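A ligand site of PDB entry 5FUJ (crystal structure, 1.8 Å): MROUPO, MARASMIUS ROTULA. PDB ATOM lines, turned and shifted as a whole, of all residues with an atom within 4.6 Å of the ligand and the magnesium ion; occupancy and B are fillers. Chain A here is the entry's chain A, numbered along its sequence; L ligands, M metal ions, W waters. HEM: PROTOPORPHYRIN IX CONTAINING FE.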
ATOM      1  N   PRO A  16     -26.855   6.192 -17.611  1.00  0.00           N
ATOM      2  CA  PRO A  16     -26.750   7.340 -16.703  1.00  0.00           C
ATOM      3  C   PRO A  16     -26.602   8.679 -17.413  1.00  0.00           C
ATOM      4  O   PRO A  16     -26.461   9.720 -16.734  1.00  0.00           O
ATOM      5  CB  PRO A  16     -25.484   7.007 -15.911  1.00  0.00           C
ATOM      6  CG  PRO A  16     -24.613   6.322 -16.948  1.00  0.00           C
ATOM      7  CD  PRO A  16     -25.590   5.438 -17.717  1.00  0.00           C
ATOM      8  N   CYS A  17     -26.558   8.647 -18.748  1.00  0.00           N
ATOM      9  CA  CYS A  17     -26.334   9.877 -19.559  1.00  0.00           C
ATOM     10  C   CYS A  17     -27.628  10.406 -20.159  1.00  0.00           C
ATOM     11  O   CYS A  17     -28.173   9.833 -21.096  1.00  0.00           O
ATOM     12  CB  CYS A  17     -25.335   9.598 -20.693  1.00  0.00           C
ATOM     13  SG  CYS A  17     -25.051  11.034 -21.758  1.00  0.00           S
ATOM     14  N   PRO A  18     -28.060  11.597 -19.727  1.00  0.00           N
ATOM     15  CA  PRO A  18     -29.223  12.177 -20.361  1.00  0.00           C
ATOM     16  C   PRO A  18     -29.006  12.519 -21.833  1.00  0.00           C
ATOM     17  O   PRO A  18     -29.965  12.578 -22.607  1.00  0.00           O
ATOM     18  CB  PRO A  18     -29.483  13.451 -19.548  1.00  0.00           C
ATOM     19  CG  PRO A  18     -28.130  13.823 -18.987  1.00  0.00           C
ATOM     20  CD  PRO A  18     -27.456  12.495 -18.712  1.00  0.00           C
ATOM     21  N   GLY A  19     -27.779  12.894 -22.204  1.00  0.00           N
ATOM     22  CA  GLY A  19     -27.519  13.246 -23.619  1.00  0.00           C
ATOM     23  C   GLY A  19     -27.829  12.069 -24.566  1.00  0.00           C
ATOM     24  O   GLY A  19     -28.583  12.217 -25.531  1.00  0.00           O
ATOM     25  N   LEU A  20     -27.264  10.903 -24.260  1.00  0.00           N
ATOM     26  CA  LEU A  20     -27.466   9.714 -25.104  1.00  0.00           C
ATOM     27  C   LEU A  20     -28.882   9.147 -24.918  1.00  0.00           C
ATOM     28  O   LEU A  20     -29.533   8.760 -25.891  1.00  0.00           O
ATOM     29  CB  LEU A  20     -26.457   8.613 -24.740  1.00  0.00           C
ATOM     30  CG  LEU A  20     -24.983   8.976 -24.992  1.00  0.00           C
ATOM     31  CD1 LEU A  20     -24.133   7.779 -24.657  1.00  0.00           C
ATOM     32  CD2 LEU A  20     -24.737   9.357 -26.458  1.00  0.00           C
ATOM     33  N   LEU A  23     -31.196  11.137 -27.105  1.00  0.00           N
ATOM     34  CA  LEU A  23     -31.091  10.807 -28.514  1.00  0.00           C
ATOM     35  C   LEU A  23     -31.824   9.474 -28.822  1.00  0.00           C
ATOM     36  O   LEU A  23     -32.428   9.363 -29.887  1.00  0.00           O
ATOM     37  CB  LEU A  23     -29.634  10.724 -28.998  1.00  0.00           C
ATOM     38  CG  LEU A  23     -28.885  12.060 -28.940  1.00  0.00           C
ATOM     39  CD1 LEU A  23     -27.365  11.815 -29.092  1.00  0.00           C
ATOM     40  CD2 LEU A  23     -29.382  13.097 -29.940  1.00  0.00           C
ATOM     41  N   ILE A  41     -23.049   7.018 -32.452  1.00  0.00           N
ATOM     42  CA  ILE A  41     -23.017   8.159 -31.536  1.00  0.00           C
ATOM     43  C   ILE A  41     -22.600   9.466 -32.208  1.00  0.00           C
ATOM     44  O   ILE A  41     -23.220  10.514 -32.007  1.00  0.00           O
ATOM     45  CB  ILE A  41     -22.099   7.859 -30.328  1.00  0.00           C
ATOM     46  CG1 ILE A  41     -22.713   6.764 -29.435  1.00  0.00           C
ATOM     47  CG2 ILE A  41     -21.847   9.163 -29.525  1.00  0.00           C
ATOM     48  CD1 ILE A  41     -21.740   6.210 -28.385  1.00  0.00           C
ATOM     49  N   GLY A  45     -25.286  12.489 -32.327  1.00  0.00           N
ATOM     50  CA  GLY A  45     -24.970  13.698 -31.589  1.00  0.00           C
ATOM     51  C   GLY A  45     -24.834  14.877 -32.530  1.00  0.00           C
ATOM     52  O   GLY A  45     -25.229  15.998 -32.189  1.00  0.00           O
ATOM     53  N   TYR A  49     -27.865  17.505 -31.893  1.00  0.00           N
ATOM     54  CA  TYR A  49     -27.398  18.585 -30.996  1.00  0.00           C
ATOM     55  C   TYR A  49     -26.370  19.505 -31.682  1.00  0.00           C
ATOM     56  O   TYR A  49     -25.949  20.502 -31.092  1.00  0.00           O
ATOM     57  CB  TYR A  49     -26.715  17.980 -29.768  1.00  0.00           C
ATOM     58  CG  TYR A  49     -27.539  17.043 -28.922  1.00  0.00           C
ATOM     59  CD1 TYR A  49     -28.880  17.328 -28.621  1.00  0.00           C
ATOM     60  CD2 TYR A  49     -26.926  15.974 -28.281  1.00  0.00           C
ATOM     61  CE1 TYR A  49     -29.583  16.521 -27.744  1.00  0.00           C
ATOM     62  CE2 TYR A  49     -27.627  15.162 -27.411  1.00  0.00           C
ATOM     63  CZ  TYR A  49     -28.972  15.437 -27.155  1.00  0.00           C
ATOM     64  OH  TYR A  49     -29.636  14.649 -26.229  1.00  0.00           O
ATOM     65  N   LEU A  56     -17.133  13.448 -29.441  1.00  0.00           N
ATOM     66  CA  LEU A  56     -17.918  12.211 -29.466  1.00  0.00           C
ATOM     67  C   LEU A  56     -17.085  10.958 -29.725  1.00  0.00           C
ATOM     68  O   LEU A  56     -17.384   9.869 -29.184  1.00  0.00           O
ATOM     69  CB  LEU A  56     -19.089  12.320 -30.438  1.00  0.00           C
ATOM     70  CG  LEU A  56     -20.094  13.408 -30.026  1.00  0.00           C
ATOM     71  CD1 LEU A  56     -21.212  13.539 -31.047  1.00  0.00           C
ATOM     72  CD2 LEU A  56     -20.689  13.097 -28.648  1.00  0.00           C
ATOM     73  N   ALA A  59     -15.042  10.586 -26.203  1.00  0.00           N
ATOM     74  CA  ALA A  59     -15.888  10.039 -25.147  1.00  0.00           C
ATOM     75  C   ALA A  59     -16.427   8.669 -25.523  1.00  0.00           C
ATOM     76  O   ALA A  59     -16.497   7.774 -24.687  1.00  0.00           O
ATOM     77  CB  ALA A  59     -17.038  10.996 -24.836  1.00  0.00           C
ATOM     78  N   GLY A  60     -16.838   8.534 -26.792  1.00  0.00           N
ATOM     79  CA  GLY A  60     -17.436   7.274 -27.274  1.00  0.00           C
ATOM     80  C   GLY A  60     -16.548   6.053 -27.150  1.00  0.00           C
ATOM     81  O   GLY A  60     -16.983   4.989 -26.691  1.00  0.00           O
ATOM     82  N   GLY A  63     -16.373   5.009 -23.624  1.00  0.00           N
ATOM     83  CA  GLY A  63     -17.636   4.364 -23.276  1.00  0.00           C
ATOM     84  C   GLY A  63     -17.733   2.932 -23.780  1.00  0.00           C
ATOM     85  O   GLY A  63     -18.355   2.090 -23.118  1.00  0.00           O
ATOM     86  N   LEU A  78     -23.142   1.853 -19.660  1.00  0.00           N
ATOM     87  CA  LEU A  78     -22.369   3.041 -19.327  1.00  0.00           C
ATOM     88  C   LEU A  78     -22.425   3.351 -17.840  1.00  0.00           C
ATOM     89  O   LEU A  78     -21.682   4.228 -17.347  1.00  0.00           O
ATOM     90  CB  LEU A  78     -22.857   4.240 -20.137  1.00  0.00           C
ATOM     91  CG  LEU A  78     -22.453   4.191 -21.618  1.00  0.00           C
ATOM     92  CD1 LEU A  78     -23.212   5.254 -22.386  1.00  0.00           C
ATOM     93  CD2 LEU A  78     -20.937   4.322 -21.821  1.00  0.00           C
ATOM     94  N   ILE A  84     -16.484   5.912 -17.090  1.00  0.00           N
ATOM     95  CA  ILE A  84     -16.933   7.317 -17.103  1.00  0.00           C
ATOM     96  C   ILE A  84     -17.841   7.638 -15.897  1.00  0.00           C
ATOM     97  O   ILE A  84     -17.682   8.674 -15.235  1.00  0.00           O
ATOM     98  CB  ILE A  84     -17.665   7.663 -18.415  1.00  0.00           C
ATOM     99  CG1 ILE A  84     -16.697   7.540 -19.592  1.00  0.00           C
ATOM    100  CG2 ILE A  84     -18.243   9.083 -18.363  1.00  0.00           C
ATOM    101  CD1 ILE A  84     -17.420   7.479 -20.929  1.00  0.00           C
ATOM    102  N   GLU A  85     -18.672   6.680 -15.504  1.00  0.00           N
ATOM    103  CA  GLU A  85     -19.673   6.979 -14.473  1.00  0.00           C
ATOM    104  C   GLU A  85     -18.930   7.275 -13.169  1.00  0.00           C
ATOM    105  O   GLU A  85     -17.955   6.618 -12.851  1.00  0.00           O
ATOM    106  CB  GLU A  85     -20.639   5.809 -14.296  1.00  0.00           C
ATOM    107  CG  GLU A  85     -21.857   6.138 -13.413  1.00  0.00           C
ATOM    108  CD  GLU A  85     -21.516   6.144 -11.922  1.00  0.00           C
ATOM    109  OE1 GLU A  85     -20.696   5.316 -11.490  1.00  0.00           O
ATOM    110  OE2 GLU A  85     -22.026   7.034 -11.176  1.00  0.00           O
ATOM    111  N   HIS A  86     -19.401   8.270 -12.423  1.00  0.00           N
ATOM    112  CA  HIS A  86     -18.650   8.821 -11.285  1.00  0.00           C
ATOM    113  C   HIS A  86     -19.609   9.236 -10.185  1.00  0.00           C
ATOM    114  O   HIS A  86     -20.784   9.542 -10.440  1.00  0.00           O
ATOM    115  CB  HIS A  86     -17.830  10.063 -11.742  1.00  0.00           C
ATOM    116  CG  HIS A  86     -18.661  11.096 -12.447  1.00  0.00           C
ATOM    117  ND1 HIS A  86     -19.581  11.896 -11.795  1.00  0.00           N
ATOM    118  CD2 HIS A  86     -18.765  11.403 -13.762  1.00  0.00           C
ATOM    119  CE1 HIS A  86     -20.195  12.658 -12.674  1.00  0.00           C
ATOM    120  NE2 HIS A  86     -19.724  12.365 -13.876  1.00  0.00           N
ATOM    121  N   ASP A  87     -19.070   9.394  -8.982  1.00  0.00           N
ATOM    122  CA  ASP A  87     -19.788  10.017  -7.869  1.00  0.00           C
ATOM    123  C   ASP A  87     -20.058  11.500  -8.074  1.00  0.00           C
ATOM    124  O   ASP A  87     -19.477  12.144  -8.973  1.00  0.00           O
ATOM    125  CB  ASP A  87     -18.991   9.787  -6.558  1.00  0.00           C
ATOM    126  CG  ASP A  87     -18.729   8.309  -6.284  1.00  0.00           C
ATOM    127  OD1 ASP A  87     -19.578   7.466  -6.656  1.00  0.00           O
ATOM    128  OD2 ASP A  87     -17.643   7.987  -5.754  1.00  0.00           O
ATOM    129  N   SER A  89     -22.732  12.977  -9.277  1.00  0.00           N
ATOM    130  CA  SER A  89     -23.573  13.314 -10.412  1.00  0.00           C
ATOM    131  C   SER A  89     -24.615  14.345 -10.047  1.00  0.00           C
ATOM    132  O   SER A  89     -24.982  14.506  -8.872  1.00  0.00           O
ATOM    133  CB  SER A  89     -24.264  12.053 -10.960  1.00  0.00           C
ATOM    134  OG  SER A  89     -23.295  11.149 -11.436  1.00  0.00           O
ATOM    135  N   LEU A  90     -25.113  14.995 -11.089  1.00  0.00           N
ATOM    136  CA  LEU A  90     -26.096  16.038 -10.965  1.00  0.00           C
ATOM    137  C   LEU A  90     -27.483  15.479 -10.714  1.00  0.00           C
ATOM    138  O   LEU A  90     -28.343  16.222 -10.268  1.00  0.00           O
ATOM    139  CB  LEU A  90     -26.150  16.880 -12.240  1.00  0.00           C
ATOM    140  CG  LEU A  90     -24.826  17.543 -12.659  1.00  0.00           C
ATOM    141  CD1 LEU A  90     -24.933  17.990 -14.110  1.00  0.00           C
ATOM    142  CD2 LEU A  90     -24.569  18.733 -11.737  1.00  0.00           C
ATOM    143  N   SER A  91     -27.738  14.234 -11.119  1.00  0.00           N
ATOM    144  CA  SER A  91     -29.133  13.749 -11.172  1.00  0.00           C
ATOM    145  C   SER A  91     -29.262  12.264 -10.870  1.00  0.00           C
ATOM    146  O   SER A  91     -30.367  11.736 -10.934  1.00  0.00           O
ATOM    147  CB  SER A  91     -29.795  14.056 -12.536  1.00  0.00           C
ATOM    148  OG  SER A  91     -29.303  13.179 -13.548  1.00  0.00           O
ATOM    149  N   ARG A  92     -28.154  11.625 -10.486  1.00  0.00           N
ATOM    150  CA  ARG A  92     -28.110  10.208 -10.080  1.00  0.00           C
ATOM    151  C   ARG A  92     -27.452  10.103  -8.696  1.00  0.00           C
ATOM    152  O   ARG A  92     -26.654  10.974  -8.321  1.00  0.00           O
ATOM    153  CB  ARG A  92     -27.286   9.383 -11.095  1.00  0.00           C
ATOM    154  CG  ARG A  92     -28.104   8.789 -12.235  1.00  0.00           C
ATOM    155  CD  ARG A  92     -28.743   9.818 -13.133  1.00  0.00           C
ATOM    156  NE  ARG A  92     -29.290   9.152 -14.332  1.00  0.00           N
ATOM    157  CZ  ARG A  92     -29.975   9.773 -15.283  1.00  0.00           C
ATOM    158  NH1 ARG A  92     -30.226  11.068 -15.174  1.00  0.00           N
ATOM    159  NH2 ARG A  92     -30.481   9.074 -16.322  1.00  0.00           N
ATOM    160  N   ASN A 100     -26.938   4.474  -9.250  1.00  0.00           N
ATOM    161  CA  ASN A 100     -26.103   5.332 -10.138  1.00  0.00           C
ATOM    162  C   ASN A 100     -26.584   5.419 -11.571  1.00  0.00           C
ATOM    163  O   ASN A 100     -25.921   6.019 -12.428  1.00  0.00           O
ATOM    164  CB  ASN A 100     -24.624   4.887 -10.098  1.00  0.00           C
ATOM    165  CG  ASN A 100     -24.355   3.612 -10.882  1.00  0.00           C
ATOM    166  OD1 ASN A 100     -25.296   2.874 -11.241  1.00  0.00           O
ATOM    167  ND2 ASN A 100     -23.074   3.357 -11.208  1.00  0.00           N
ATOM    168  N   GLU A 157     -19.581  17.561 -18.355  1.00  0.00           N
ATOM    169  CA  GLU A 157     -21.025  17.295 -18.376  1.00  0.00           C
ATOM    170  C   GLU A 157     -21.886  18.523 -18.121  1.00  0.00           C
ATOM    171  O   GLU A 157     -22.886  18.731 -18.822  1.00  0.00           O
ATOM    172  CB  GLU A 157     -21.370  16.099 -17.459  1.00  0.00           C
ATOM    173  CG  GLU A 157     -20.773  14.806 -18.035  1.00  0.00           C
ATOM    174  CD  GLU A 157     -20.537  13.679 -17.035  1.00  0.00           C
ATOM    175  OE1 GLU A 157     -20.678  13.891 -15.806  1.00  0.00           O
ATOM    176  OE2 GLU A 157     -20.104  12.591 -17.464  1.00  0.00           O
ATOM    177  N   PHE A 160     -21.704  20.443 -21.177  1.00  0.00           N
ATOM    178  CA  PHE A 160     -22.595  19.829 -22.174  1.00  0.00           C
ATOM    179  C   PHE A 160     -24.037  20.354 -22.034  1.00  0.00           C
ATOM    180  O   PHE A 160     -24.656  20.738 -23.013  1.00  0.00           O
ATOM    181  CB  PHE A 160     -22.570  18.284 -22.086  1.00  0.00           C
ATOM    182  CG  PHE A 160     -21.814  17.628 -23.201  1.00  0.00           C
ATOM    183  CD1 PHE A 160     -21.816  18.177 -24.481  1.00  0.00           C
ATOM    184  CD2 PHE A 160     -21.199  16.397 -23.011  1.00  0.00           C
ATOM    185  CE1 PHE A 160     -21.177  17.542 -25.531  1.00  0.00           C
ATOM    186  CE2 PHE A 160     -20.505  15.779 -24.046  1.00  0.00           C
ATOM    187  CZ  PHE A 160     -20.530  16.345 -25.318  1.00  0.00           C
ATOM    188  N   PHE A 161     -24.597  20.305 -20.830  1.00  0.00           N
ATOM    189  CA  PHE A 161     -26.017  20.693 -20.714  1.00  0.00           C
ATOM    190  C   PHE A 161     -26.195  22.211 -20.903  1.00  0.00           C
ATOM    191  O   PHE A 161     -27.166  22.655 -21.536  1.00  0.00           O
ATOM    192  CB  PHE A 161     -26.696  20.146 -19.433  1.00  0.00           C
ATOM    193  CG  PHE A 161     -26.510  21.001 -18.208  1.00  0.00           C
ATOM    194  CD1 PHE A 161     -27.095  22.281 -18.123  1.00  0.00           C
ATOM    195  CD2 PHE A 161     -25.781  20.531 -17.124  1.00  0.00           C
ATOM    196  CE1 PHE A 161     -26.928  23.054 -16.996  1.00  0.00           C
ATOM    197  CE2 PHE A 161     -25.612  21.299 -15.982  1.00  0.00           C
ATOM    198  CZ  PHE A 161     -26.199  22.564 -15.924  1.00  0.00           C
ATOM    199  N   VAL A 164     -25.612  22.401 -25.127  1.00  0.00           N
ATOM    200  CA  VAL A 164     -26.550  21.670 -25.993  1.00  0.00           C
ATOM    201  C   VAL A 164     -28.014  22.162 -25.798  1.00  0.00           C
ATOM    202  O   VAL A 164     -28.802  22.244 -26.777  1.00  0.00           O
ATOM    203  CB  VAL A 164     -26.416  20.165 -25.775  1.00  0.00           C
ATOM    204  CG1 VAL A 164     -27.555  19.392 -26.406  1.00  0.00           C
ATOM    205  CG2 VAL A 164     -25.079  19.685 -26.342  1.00  0.00           C
ATOM    206  N   PHE A 183     -34.899  18.293 -20.348  1.00  0.00           N
ATOM    207  CA  PHE A 183     -33.768  17.413 -20.719  1.00  0.00           C
ATOM    208  C   PHE A 183     -33.455  16.342 -19.661  1.00  0.00           C
ATOM    209  O   PHE A 183     -33.367  15.162 -19.987  1.00  0.00           O
ATOM    210  CB  PHE A 183     -32.534  18.301 -20.995  1.00  0.00           C
ATOM    211  CG  PHE A 183     -31.300  17.552 -21.441  1.00  0.00           C
ATOM    212  CD1 PHE A 183     -31.228  16.967 -22.706  1.00  0.00           C
ATOM    213  CD2 PHE A 183     -30.161  17.542 -20.637  1.00  0.00           C
ATOM    214  CE1 PHE A 183     -30.060  16.318 -23.103  1.00  0.00           C
ATOM    215  CE2 PHE A 183     -28.987  16.964 -21.057  1.00  0.00           C
ATOM    216  CZ  PHE A 183     -28.930  16.330 -22.291  1.00  0.00           C
ATOM    217  N   PHE A 184     -33.226  16.749 -18.410  1.00  0.00           N
ATOM    218  CA  PHE A 184     -32.921  15.802 -17.315  1.00  0.00           C
ATOM    219  C   PHE A 184     -34.132  14.936 -16.909  1.00  0.00           C
ATOM    220  O   PHE A 184     -34.022  13.706 -16.829  1.00  0.00           O
ATOM    221  CB  PHE A 184     -32.395  16.536 -16.082  1.00  0.00           C
ATOM    222  CG  PHE A 184     -30.908  16.824 -16.115  1.00  0.00           C
ATOM    223  CD1 PHE A 184     -29.991  15.902 -15.651  1.00  0.00           C
ATOM    224  CD2 PHE A 184     -30.451  18.029 -16.640  1.00  0.00           C
ATOM    225  CE1 PHE A 184     -28.621  16.176 -15.683  1.00  0.00           C
ATOM    226  CE2 PHE A 184     -29.101  18.313 -16.672  1.00  0.00           C
ATOM    227  CZ  PHE A 184     -28.186  17.397 -16.176  1.00  0.00           C
HETATM  228  CHA HEM L   1     -23.434  11.869 -17.903  1.00  0.00           C
HETATM  229  CHB HEM L   1     -24.691  15.040 -21.366  1.00  0.00           C
HETATM  230  CHC HEM L   1     -22.476  12.140 -24.675  1.00  0.00           C
HETATM  231  CHD HEM L   1     -21.437   8.905 -21.193  1.00  0.00           C
HETATM  232  C1A HEM L   1     -23.831  13.008 -18.555  1.00  0.00           C
HETATM  233  C2A HEM L   1     -24.383  14.147 -17.896  1.00  0.00           C
HETATM  234  C3A HEM L   1     -24.732  15.042 -18.854  1.00  0.00           C
HETATM  235  C4A HEM L   1     -24.417  14.470 -20.119  1.00  0.00           C
HETATM  236  CMA HEM L   1     -25.345  16.410 -18.612  1.00  0.00           C
HETATM  237  CAA HEM L   1     -24.468  14.331 -16.391  1.00  0.00           C
HETATM  238  CBA HEM L   1     -25.610  13.512 -15.746  1.00  0.00           C
HETATM  239  CGA HEM L   1     -25.580  13.715 -14.234  1.00  0.00           C
HETATM  240  O1A HEM L   1     -26.607  13.427 -13.564  1.00  0.00           O
HETATM  241  O2A HEM L   1     -24.557  14.189 -13.640  1.00  0.00           O
HETATM  242  C1B HEM L   1     -24.232  14.457 -22.582  1.00  0.00           C
HETATM  243  C2B HEM L   1     -24.458  15.060 -23.863  1.00  0.00           C
HETATM  244  C3B HEM L   1     -23.894  14.250 -24.801  1.00  0.00           C
HETATM  245  C4B HEM L   1     -23.275  13.136 -24.076  1.00  0.00           C
HETATM  246  CMB HEM L   1     -25.255  16.313 -24.160  1.00  0.00           C
HETATM  247  CAB HEM L   1     -23.895  14.509 -26.265  1.00  0.00           C
HETATM  248  CBB HEM L   1     -24.182  13.510 -27.117  1.00  0.00           C
HETATM  249  C1C HEM L   1     -21.880  11.077 -23.993  1.00  0.00           C
HETATM  250  C2C HEM L   1     -21.081  10.081 -24.593  1.00  0.00           C
HETATM  251  C3C HEM L   1     -20.811   9.139 -23.613  1.00  0.00           C
HETATM  252  C4C HEM L   1     -21.456   9.583 -22.392  1.00  0.00           C
HETATM  253  CMC HEM L   1     -20.663  10.108 -26.061  1.00  0.00           C
HETATM  254  CAC HEM L   1     -20.024   7.891 -23.725  1.00  0.00           C
HETATM  255  CBC HEM L   1     -20.222   7.087 -24.776  1.00  0.00           C
HETATM  256  C1D HEM L   1     -21.932   9.514 -20.031  1.00  0.00           C
HETATM  257  C2D HEM L   1     -21.886   8.794 -18.745  1.00  0.00           C
HETATM  258  C3D HEM L   1     -22.385   9.632 -17.833  1.00  0.00           C
HETATM  259  C4D HEM L   1     -22.828  10.816 -18.581  1.00  0.00           C
HETATM  260  CMD HEM L   1     -21.257   7.447 -18.481  1.00  0.00           C
HETATM  261  CAD HEM L   1     -22.527   9.329 -16.355  1.00  0.00           C
HETATM  262  CBD HEM L   1     -21.521  10.201 -15.556  1.00  0.00           C
HETATM  263  CGD HEM L   1     -22.133  10.383 -14.165  1.00  0.00           C
HETATM  264  O1D HEM L   1     -21.799   9.591 -13.285  1.00  0.00           O
HETATM  265  O2D HEM L   1     -22.924  11.332 -13.895  1.00  0.00           O
HETATM  266  NA  HEM L   1     -23.852  13.192 -19.923  1.00  0.00           N
HETATM  267  NB  HEM L   1     -23.515  13.314 -22.751  1.00  0.00           N
HETATM  268  NC  HEM L   1     -22.095  10.743 -22.665  1.00  0.00           N
HETATM  269  ND  HEM L   1     -22.520  10.731 -19.902  1.00  0.00           N
HETATM  270 FE   HEM L   1     -23.000  11.976 -21.257  1.00  0.00          FE
HETATM  271 MG    MG M   1     -22.687   9.070 -11.381  1.00  0.00          MG
HETATM  272  O   HOH W   1     -24.369   8.387 -12.497  1.00  0.00           O
HETATM  273  O   HOH W   2     -22.030  15.168 -13.717  1.00  0.00           O
HETATM  274  O   HOH W   3     -25.507  10.133 -14.132  1.00  0.00           O
HETATM  275  O   HOH W   4     -23.583   8.918  -9.499  1.00  0.00           O
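The magnesium ion is bound by water W4 (2.1 Å), water W1 (2.1 Å), OE2 of Glu 85 (2.2 Å), O1D of the ligand (2.2 Å), OG of Ser 89 (2.2 Å) and O of His 86 (2.2 Å). The magnesium ion has six donor atoms within binding distance.
OH of Tyr 49 sits at hydrogen-bond distance from O of Gly 19, 2.7 Å away. OE1 of Glu 85 lies within hydrogen-bond range of ND2 of Asn 100. SG of Cys 17 lies close to N of Gly 19, at 3.3 Å. OG of Ser 91 sits at hydrogen-bond distance from NH1 of Arg 92 (2.8 Å). N of Leu 20 lies close to SG of Cys 17. A ring nitrogen (NE2) of His 86 lies within hydrogen-bond range of the side-chain carboxylate (OE1) of Glu 157 (2.6 Å).
Merely in contact with the ligand: Pro 16, Pro 18, Gly 19, Leu 20, Ile 41, Tyr 49, Leu 56, Ala 59, Gly 60, Leu 78, Ile 84, Arg 92, Glu 157, Phe 160 and Phe 184. Hydrophobic or aromatic side chains that line the ligand: Pro 16, Pro 18, Leu 20, Ile 41, Tyr 49, Leu 56, Ala 59, Leu 78, Ile 84, His 86, Leu 90, Phe 160 and Phe 184. Within 4 Å of the ligand: Pro 16, Cys 17, Pro 18, Gly 19, Leu 20, Ile 41, Tyr 49, Leu 56, Ala 59, Gly 60, Leu 78, Ile 84, Glu 85, His 86, Ser 89, Leu 90, Ser 91, Arg 92, Glu 157, Phe 160 and Phe 184. The nearest printed residue that does not touch the ligand is Val 164 (4.02 Å).
The backbone NH (N) of His 86 lies close to an oxygen (O1D) of the ligand (2.9 Å). N of Leu 90 is in hydrogen-bond range of O2A of the ligand (2.7 Å). O2D of the ligand sits close to NE2 of His 86, at 3.4 Å. An oxygen (O1A) of the ligand is in hydrogen-bond range of the backbone NH (N) of Ser 91. An oxygen (O1A) of the ligand sits at hydrogen-bond distance from the side-chain hydroxyl (OG) of Ser 91. An iron atom (FE) of the ligand is bound by the side-chain sulfur of Cys 17, at 2.3 Å.
Water W2 lies within hydrogen-bond range of an oxygen (O2A) of the ligand (2.7 Å) and the side-chain carboxylate of Glu 157 (2.8 Å). Water W3 lies within hydrogen-bond range of the backbone carbonyl oxygen (O) of Pro 16 (2.8 Å) and an oxygen (O2D) of the ligand (2.9 Å).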
